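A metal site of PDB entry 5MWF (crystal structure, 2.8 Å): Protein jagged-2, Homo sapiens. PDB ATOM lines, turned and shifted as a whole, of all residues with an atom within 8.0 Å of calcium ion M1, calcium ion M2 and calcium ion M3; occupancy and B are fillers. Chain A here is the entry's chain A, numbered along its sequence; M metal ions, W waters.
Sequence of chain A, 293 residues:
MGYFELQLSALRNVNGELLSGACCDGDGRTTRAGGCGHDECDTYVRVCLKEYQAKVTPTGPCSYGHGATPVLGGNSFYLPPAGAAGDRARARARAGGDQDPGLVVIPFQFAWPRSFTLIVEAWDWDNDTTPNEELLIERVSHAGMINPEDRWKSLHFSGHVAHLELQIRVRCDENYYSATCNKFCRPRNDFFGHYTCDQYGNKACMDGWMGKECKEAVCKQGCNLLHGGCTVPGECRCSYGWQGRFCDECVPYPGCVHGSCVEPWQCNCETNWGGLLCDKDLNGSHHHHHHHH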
ATOM      1  N   LEU A  18     -12.193  22.745  -4.922  1.00  0.00           N
ATOM      2  CA  LEU A  18     -10.748  22.862  -4.909  1.00  0.00           C
ATOM      3  C   LEU A  18     -10.351  23.842  -5.995  1.00  0.00           C
ATOM      4  O   LEU A  18     -11.181  24.297  -6.779  1.00  0.00           O
ATOM      5  CB  LEU A  18     -10.074  21.498  -5.118  1.00  0.00           C
ATOM      6  CG  LEU A  18     -10.477  20.373  -4.158  1.00  0.00           C
ATOM      7  CD1 LEU A  18     -10.177  19.012  -4.767  1.00  0.00           C
ATOM      8  CD2 LEU A  18      -9.789  20.523  -2.824  1.00  0.00           C
ATOM      9  N   CYS A  23     -15.130  18.973  -6.401  1.00  0.00           N
ATOM     10  CA  CYS A  23     -15.504  19.082  -5.008  1.00  0.00           C
ATOM     11  C   CYS A  23     -14.437  18.437  -4.140  1.00  0.00           C
ATOM     12  O   CYS A  23     -13.719  17.529  -4.562  1.00  0.00           O
ATOM     13  CB  CYS A  23     -16.870  18.419  -4.760  1.00  0.00           C
ATOM     14  SG  CYS A  23     -18.275  19.091  -5.699  1.00  0.00           S
ATOM     15  N   CYS A  24     -14.334  18.925  -2.898  1.00  0.00           N
ATOM     16  CA  CYS A  24     -13.263  18.485  -2.006  1.00  0.00           C
ATOM     17  C   CYS A  24     -13.333  16.979  -1.757  1.00  0.00           C
ATOM     18  O   CYS A  24     -12.356  16.253  -1.998  1.00  0.00           O
ATOM     19  CB  CYS A  24     -13.335  19.247  -0.680  1.00  0.00           C
ATOM     20  SG  CYS A  24     -12.664  20.914  -0.706  1.00  0.00           S
ATOM     21  N   ASP A  25     -14.482  16.506  -1.285  1.00  0.00           N
ATOM     22  CA  ASP A  25     -14.667  15.099  -0.945  1.00  0.00           C
ATOM     23  C   ASP A  25     -15.867  14.581  -1.727  1.00  0.00           C
ATOM     24  O   ASP A  25     -17.008  14.906  -1.408  1.00  0.00           O
ATOM     25  CB  ASP A  25     -14.863  14.914   0.560  1.00  0.00           C
ATOM     26  CG  ASP A  25     -13.605  15.201   1.349  1.00  0.00           C
ATOM     27  OD1 ASP A  25     -12.503  15.127   0.775  1.00  0.00           O
ATOM     28  OD2 ASP A  25     -13.715  15.493   2.563  1.00  0.00           O
ATOM     29  N   GLY A  26     -15.594  13.788  -2.755  1.00  0.00           N
ATOM     30  CA  GLY A  26     -16.651  13.217  -3.548  1.00  0.00           C
ATOM     31  C   GLY A  26     -16.444  13.365  -5.037  1.00  0.00           C
ATOM     32  O   GLY A  26     -16.072  14.436  -5.522  1.00  0.00           O
ATOM     33  N   HIS A  38     -22.790  17.175   1.496  1.00  0.00           N
ATOM     34  CA  HIS A  38     -22.625  17.391   2.929  1.00  0.00           C
ATOM     35  C   HIS A  38     -21.251  17.002   3.444  1.00  0.00           C
ATOM     36  O   HIS A  38     -20.878  17.440   4.530  1.00  0.00           O
ATOM     37  CB  HIS A  38     -23.670  16.602   3.725  1.00  0.00           C
ATOM     38  CG  HIS A  38     -25.071  17.131   3.598  1.00  0.00           C
ATOM     39  ND1 HIS A  38     -26.104  16.675   4.387  1.00  0.00           N
ATOM     40  CD2 HIS A  38     -25.599  18.066   2.788  1.00  0.00           C
ATOM     41  CE1 HIS A  38     -27.217  17.322   4.067  1.00  0.00           C
ATOM     42  NE2 HIS A  38     -26.930  18.165   3.093  1.00  0.00           N
ATOM     43  N   ASP A  39     -20.488  16.214   2.688  1.00  0.00           N
ATOM     44  CA  ASP A  39     -19.083  15.992   3.039  1.00  0.00           C
ATOM     45  C   ASP A  39     -18.308  17.223   2.581  1.00  0.00           C
ATOM     46  O   ASP A  39     -17.991  17.368   1.403  1.00  0.00           O
ATOM     47  CB  ASP A  39     -18.557  14.715   2.402  1.00  0.00           C
ATOM     48  CG  ASP A  39     -17.279  14.230   3.060  1.00  0.00           C
ATOM     49  OD1 ASP A  39     -16.568  15.060   3.663  1.00  0.00           O
ATOM     50  OD2 ASP A  39     -16.981  13.019   2.966  1.00  0.00           O
ATOM     51  N   GLU A  40     -18.001  18.109   3.523  1.00  0.00           N
ATOM     52  CA  GLU A  40     -17.368  19.375   3.237  1.00  0.00           C
ATOM     53  C   GLU A  40     -15.840  19.233   3.179  1.00  0.00           C
ATOM     54  O   GLU A  40     -15.282  18.169   3.444  1.00  0.00           O
ATOM     55  CB  GLU A  40     -17.752  20.431   4.286  1.00  0.00           C
ATOM     56  CG  GLU A  40     -19.244  20.668   4.415  1.00  0.00           C
ATOM     57  CD  GLU A  40     -19.575  21.756   5.416  1.00  0.00           C
ATOM     58  OE1 GLU A  40     -20.464  22.591   5.122  1.00  0.00           O
ATOM     59  OE2 GLU A  40     -18.953  21.792   6.501  1.00  0.00           O
ATOM     60  N   CYS A  41     -15.190  20.323   2.799  1.00  0.00           N
ATOM     61  CA  CYS A  41     -13.728  20.375   2.820  1.00  0.00           C
ATOM     62  C   CYS A  41     -13.233  20.282   4.251  1.00  0.00           C
ATOM     63  O   CYS A  41     -13.798  20.887   5.168  1.00  0.00           O
ATOM     64  CB  CYS A  41     -13.220  21.653   2.172  1.00  0.00           C
ATOM     65  SG  CYS A  41     -13.885  21.964   0.533  1.00  0.00           S
ATOM     66  N   ASP A  42     -12.183  19.494   4.455  1.00  0.00           N
ATOM     67  CA  ASP A  42     -11.522  19.357   5.758  1.00  0.00           C
ATOM     68  C   ASP A  42     -10.285  20.258   5.717  1.00  0.00           C
ATOM     69  O   ASP A  42      -9.177  19.822   5.397  1.00  0.00           O
ATOM     70  CB  ASP A  42     -11.180  17.891   6.006  1.00  0.00           C
ATOM     71  CG  ASP A  42     -12.384  16.981   5.801  1.00  0.00           C
ATOM     72  OD1 ASP A  42     -13.500  17.379   6.225  1.00  0.00           O
ATOM     73  OD2 ASP A  42     -12.254  15.904   5.172  1.00  0.00           O
ATOM     74  N   THR A  43     -10.482  21.526   6.061  1.00  0.00           N
ATOM     75  CA  THR A  43      -9.549  22.587   5.697  1.00  0.00           C
ATOM     76  C   THR A  43      -8.477  22.794   6.755  1.00  0.00           C
ATOM     77  O   THR A  43      -8.789  22.983   7.933  1.00  0.00           O
ATOM     78  CB  THR A  43     -10.295  23.898   5.469  1.00  0.00           C
ATOM     79  OG1 THR A  43     -11.300  23.720   4.460  1.00  0.00           O
ATOM     80  CG2 THR A  43      -9.334  24.988   5.012  1.00  0.00           C
ATOM     81  N   VAL A  71      -6.851  20.449  11.004  1.00  0.00           N
ATOM     82  CA  VAL A  71      -8.094  20.831  10.364  1.00  0.00           C
ATOM     83  C   VAL A  71      -8.821  21.833  11.247  1.00  0.00           C
ATOM     84  O   VAL A  71      -9.145  21.540  12.409  1.00  0.00           O
ATOM     85  CB  VAL A  71      -8.974  19.600  10.088  1.00  0.00           C
ATOM     86  CG1 VAL A  71     -10.340  20.038   9.579  1.00  0.00           C
ATOM     87  CG2 VAL A  71      -8.302  18.699   9.067  1.00  0.00           C
ATOM     88  N   GLY A  73     -11.756  23.596  10.209  1.00  0.00           N
ATOM     89  CA  GLY A  73     -13.191  23.603  10.025  1.00  0.00           C
ATOM     90  C   GLY A  73     -13.599  23.020   8.683  1.00  0.00           C
ATOM     91  O   GLY A  73     -12.868  22.230   8.078  1.00  0.00           O
ATOM     92  N   GLY A  74     -14.780  23.420   8.231  1.00  0.00           N
ATOM     93  CA  GLY A  74     -15.332  22.916   6.992  1.00  0.00           C
ATOM     94  C   GLY A  74     -15.095  23.826   5.810  1.00  0.00           C
ATOM     95  O   GLY A  74     -13.992  24.322   5.613  1.00  0.00           O
ATOM     96  N   ASN A  75     -16.145  24.070   5.020  1.00  0.00           N
ATOM     97  CA  ASN A  75     -16.005  24.923   3.848  1.00  0.00           C
ATOM     98  C   ASN A  75     -15.778  26.377   4.242  1.00  0.00           C
ATOM     99  O   ASN A  75     -14.993  27.081   3.592  1.00  0.00           O
ATOM    100  CB  ASN A  75     -17.232  24.807   2.959  1.00  0.00           C
ATOM    101  CG  ASN A  75     -17.431  23.412   2.421  1.00  0.00           C
ATOM    102  OD1 ASN A  75     -16.482  22.626   2.325  1.00  0.00           O
ATOM    103  ND2 ASN A  75     -18.671  23.083   2.070  1.00  0.00           N
ATOM    104  N   TRP A 123      -5.625  23.609   2.271  1.00  0.00           N
ATOM    105  CA  TRP A 123      -5.609  22.246   1.773  1.00  0.00           C
ATOM    106  C   TRP A 123      -6.764  21.437   2.356  1.00  0.00           C
ATOM    107  O   TRP A 123      -7.207  21.679   3.479  1.00  0.00           O
ATOM    108  CB  TRP A 123      -4.286  21.540   2.119  1.00  0.00           C
ATOM    109  CG  TRP A 123      -3.073  22.071   1.420  1.00  0.00           C
ATOM    110  CD1 TRP A 123      -2.318  23.146   1.791  1.00  0.00           C
ATOM    111  CD2 TRP A 123      -2.478  21.557   0.231  1.00  0.00           C
ATOM    112  NE1 TRP A 123      -1.274  23.327   0.905  1.00  0.00           N
ATOM    113  CE2 TRP A 123      -1.359  22.353  -0.060  1.00  0.00           C
ATOM    114  CE3 TRP A 123      -2.784  20.484  -0.619  1.00  0.00           C
ATOM    115  CZ2 TRP A 123      -0.545  22.125  -1.172  1.00  0.00           C
ATOM    116  CZ3 TRP A 123      -1.969  20.255  -1.713  1.00  0.00           C
ATOM    117  CH2 TRP A 123      -0.867  21.073  -1.980  1.00  0.00           C
ATOM    118  N   ASP A 124      -7.235  20.466   1.565  1.00  0.00           N
ATOM    119  CA  ASP A 124      -8.197  19.476   2.031  1.00  0.00           C
ATOM    120  C   ASP A 124      -7.462  18.269   2.588  1.00  0.00           C
ATOM    121  O   ASP A 124      -6.457  17.812   2.030  1.00  0.00           O
ATOM    122  CB  ASP A 124      -9.131  19.040   0.888  1.00  0.00           C
ATOM    123  CG  ASP A 124     -10.093  17.930   1.298  1.00  0.00           C
ATOM    124  OD1 ASP A 124     -10.545  17.903   2.460  1.00  0.00           O
ATOM    125  OD2 ASP A 124     -10.405  17.064   0.443  1.00  0.00           O
ATOM    126  N   TRP A 125      -7.979  17.751   3.702  1.00  0.00           N
ATOM    127  CA  TRP A 125      -7.365  16.648   4.438  1.00  0.00           C
ATOM    128  C   TRP A 125      -8.178  15.382   4.214  1.00  0.00           C
ATOM    129  O   TRP A 125      -9.408  15.392   4.395  1.00  0.00           O
ATOM    130  CB  TRP A 125      -7.264  16.988   5.925  1.00  0.00           C
ATOM    131  CG  TRP A 125      -6.651  15.930   6.783  1.00  0.00           C
ATOM    132  CD1 TRP A 125      -7.264  15.190   7.745  1.00  0.00           C
ATOM    133  CD2 TRP A 125      -5.291  15.488   6.759  1.00  0.00           C
ATOM    134  NE1 TRP A 125      -6.392  14.320   8.322  1.00  0.00           N
ATOM    135  CE2 TRP A 125      -5.159  14.478   7.736  1.00  0.00           C
ATOM    136  CE3 TRP A 125      -4.161  15.843   6.001  1.00  0.00           C
ATOM    137  CZ2 TRP A 125      -3.957  13.820   7.975  1.00  0.00           C
ATOM    138  CZ3 TRP A 125      -2.967  15.185   6.247  1.00  0.00           C
ATOM    139  CH2 TRP A 125      -2.875  14.192   7.221  1.00  0.00           C
ATOM    140  N   ASP A 126      -7.495  14.306   3.823  1.00  0.00           N
ATOM    141  CA  ASP A 126      -8.122  13.003   3.656  1.00  0.00           C
ATOM    142  C   ASP A 126      -7.392  11.925   4.455  1.00  0.00           C
ATOM    143  O   ASP A 126      -7.324  10.768   4.024  1.00  0.00           O
ATOM    144  CB  ASP A 126      -8.210  12.606   2.173  1.00  0.00           C
ATOM    145  CG  ASP A 126      -8.885  13.660   1.318  1.00  0.00           C
ATOM    146  OD1 ASP A 126      -9.839  14.314   1.798  1.00  0.00           O
ATOM    147  OD2 ASP A 126      -8.494  13.814   0.135  1.00  0.00           O
ATOM    148  N   ASN A 127      -6.855  12.290   5.620  1.00  0.00           N
ATOM    149  CA  ASN A 127      -6.218  11.350   6.533  1.00  0.00           C
ATOM    150  C   ASN A 127      -5.137  10.530   5.837  1.00  0.00           C
ATOM    151  O   ASN A 127      -5.036   9.311   6.010  1.00  0.00           O
ATOM    152  CB  ASN A 127      -7.254  10.452   7.204  1.00  0.00           C
ATOM    153  CG  ASN A 127      -8.184  11.226   8.121  1.00  0.00           C
ATOM    154  OD1 ASN A 127      -9.232  11.694   7.686  1.00  0.00           O
ATOM    155  ND2 ASN A 127      -7.789  11.373   9.381  1.00  0.00           N
ATOM    156  N   ASN A 132      -0.215  15.331  -2.345  1.00  0.00           N
ATOM    157  CA  ASN A 132      -1.166  15.243  -3.453  1.00  0.00           C
ATOM    158  C   ASN A 132      -1.570  16.661  -3.838  1.00  0.00           C
ATOM    159  O   ASN A 132      -2.449  17.255  -3.196  1.00  0.00           O
ATOM    160  CB  ASN A 132      -2.369  14.401  -3.071  1.00  0.00           C
ATOM    161  CG  ASN A 132      -3.298  14.115  -4.250  1.00  0.00           C
ATOM    162  OD1 ASN A 132      -3.199  14.755  -5.300  1.00  0.00           O
ATOM    163  ND2 ASN A 132      -4.213  13.178  -4.063  1.00  0.00           N
ATOM    164  N   GLU A 134      -3.385  17.873  -5.954  1.00  0.00           N
ATOM    165  CA  GLU A 134      -4.760  18.075  -6.394  1.00  0.00           C
ATOM    166  C   GLU A 134      -5.711  18.362  -5.250  1.00  0.00           C
ATOM    167  O   GLU A 134      -6.901  18.573  -5.493  1.00  0.00           O
ATOM    168  CB  GLU A 134      -5.234  16.850  -7.188  1.00  0.00           C
ATOM    169  CG  GLU A 134      -4.339  16.547  -8.370  1.00  0.00           C
ATOM    170  CD  GLU A 134      -5.091  16.006  -9.551  1.00  0.00           C
ATOM    171  OE1 GLU A 134      -4.824  14.848  -9.942  1.00  0.00           O
ATOM    172  OE2 GLU A 134      -5.957  16.740 -10.081  1.00  0.00           O
ATOM    173  N   LEU A 135      -5.221  18.361  -4.007  1.00  0.00           N
ATOM    174  CA  LEU A 135      -6.028  18.707  -2.845  1.00  0.00           C
ATOM    175  C   LEU A 135      -5.882  20.167  -2.441  1.00  0.00           C
ATOM    176  O   LEU A 135      -6.279  20.541  -1.333  1.00  0.00           O
ATOM    177  CB  LEU A 135      -5.680  17.789  -1.671  1.00  0.00           C
ATOM    178  CG  LEU A 135      -5.687  16.280  -1.964  1.00  0.00           C
ATOM    179  CD1 LEU A 135      -4.969  15.534  -0.853  1.00  0.00           C
ATOM    180  CD2 LEU A 135      -7.109  15.775  -2.130  1.00  0.00           C
HETATM  181 CA    CA M   1     -14.727  16.151   4.564  1.00  0.00          CA
HETATM  182 CA    CA M   2     -11.279  15.541   2.883  1.00  0.00          CA
HETATM  183 CA    CA M   3     -10.576  14.771  -0.543  1.00  0.00          CA
HETATM  184  O   HOH W   1     -12.068  12.476  -2.432  1.00  0.00           O
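Within 4 Å of calcium ion M1: Asp 25, Asp 39, Glu 40 and Asp 42.
OD1 of Asp 39 is bound to calcium ion M1, 2.3 Å away. Calcium ion M1 is bound by OD2 of Asp 25. Calcium ion M1 is bound by the backbone carbonyl oxygen (O) of Glu 40 (2.4 Å). Calcium ion M1 is bound by OD1 of Asp 42 (2.4 Å). Calcium ion M1 is bound by OD2 of Asp 42, at 2.6 Å.
Of the 23 residues printed, 5 come within 4 Å of calcium ion M2. The nearest printed residue that does not touch calcium ion M2 is Glu 40 (4.8 Å).
Merely in contact with calcium ion M3: Leu 135. Within 4 Å of calcium ion M3: Cys 24, Asp 25, Asp 124, Asp 126 and Leu 135. The nearest printed residue that does not touch calcium ion M3 is Trp 125 (5.1 Å).
NE1 of Trp 125 lies close to ND2 of Asn 127, at 3.4 Å. The backbone carbonyl oxygen (O) of Leu 135 sits at hydrogen-bond distance from the backbone NH (N) of Asp 124 (3.1 Å). The side-chain sulfur of Cys 41 forms a disulfide with the side-chain sulfur of Cys 24, at 2.0 Å.
Calcium ion M3 is bound by the side-chain carboxylate (OD1) of Asp 25 (2.4 Å), the side-chain carboxylate (OD2) of Asp 126 (2.4 Å), the side-chain carboxylate (OD1) of Asp 126 (2.5 Å), the side-chain carboxylate (OD2) of Asp 124 (2.5 Å) and the backbone carbonyl oxygen (O) of Cys 24 (2.7 Å). Calcium ion M3 has five donor atoms within binding distance.
Calcium ion M2 is bound by the side-chain carboxylate (OD1) of Asp 126 (2.2 Å), the backbone carbonyl oxygen (O) of Trp 125 (2.4 Å), the side-chain carboxylate (OD2) of Asp 25 (2.5 Å), the side-chain carboxylate (OD1) of Asp 25 (2.5 Å), the side-chain carboxylate (OD1) of Asp 124 (2.5 Å) and the side-chain carboxylate (OD2) of Asp 42 (2.5 Å). Calcium ion M2 has six donor atoms within binding distance. Slightly farther from calcium ion M2 lies OD2 of Asp 124 (3.0 Å).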
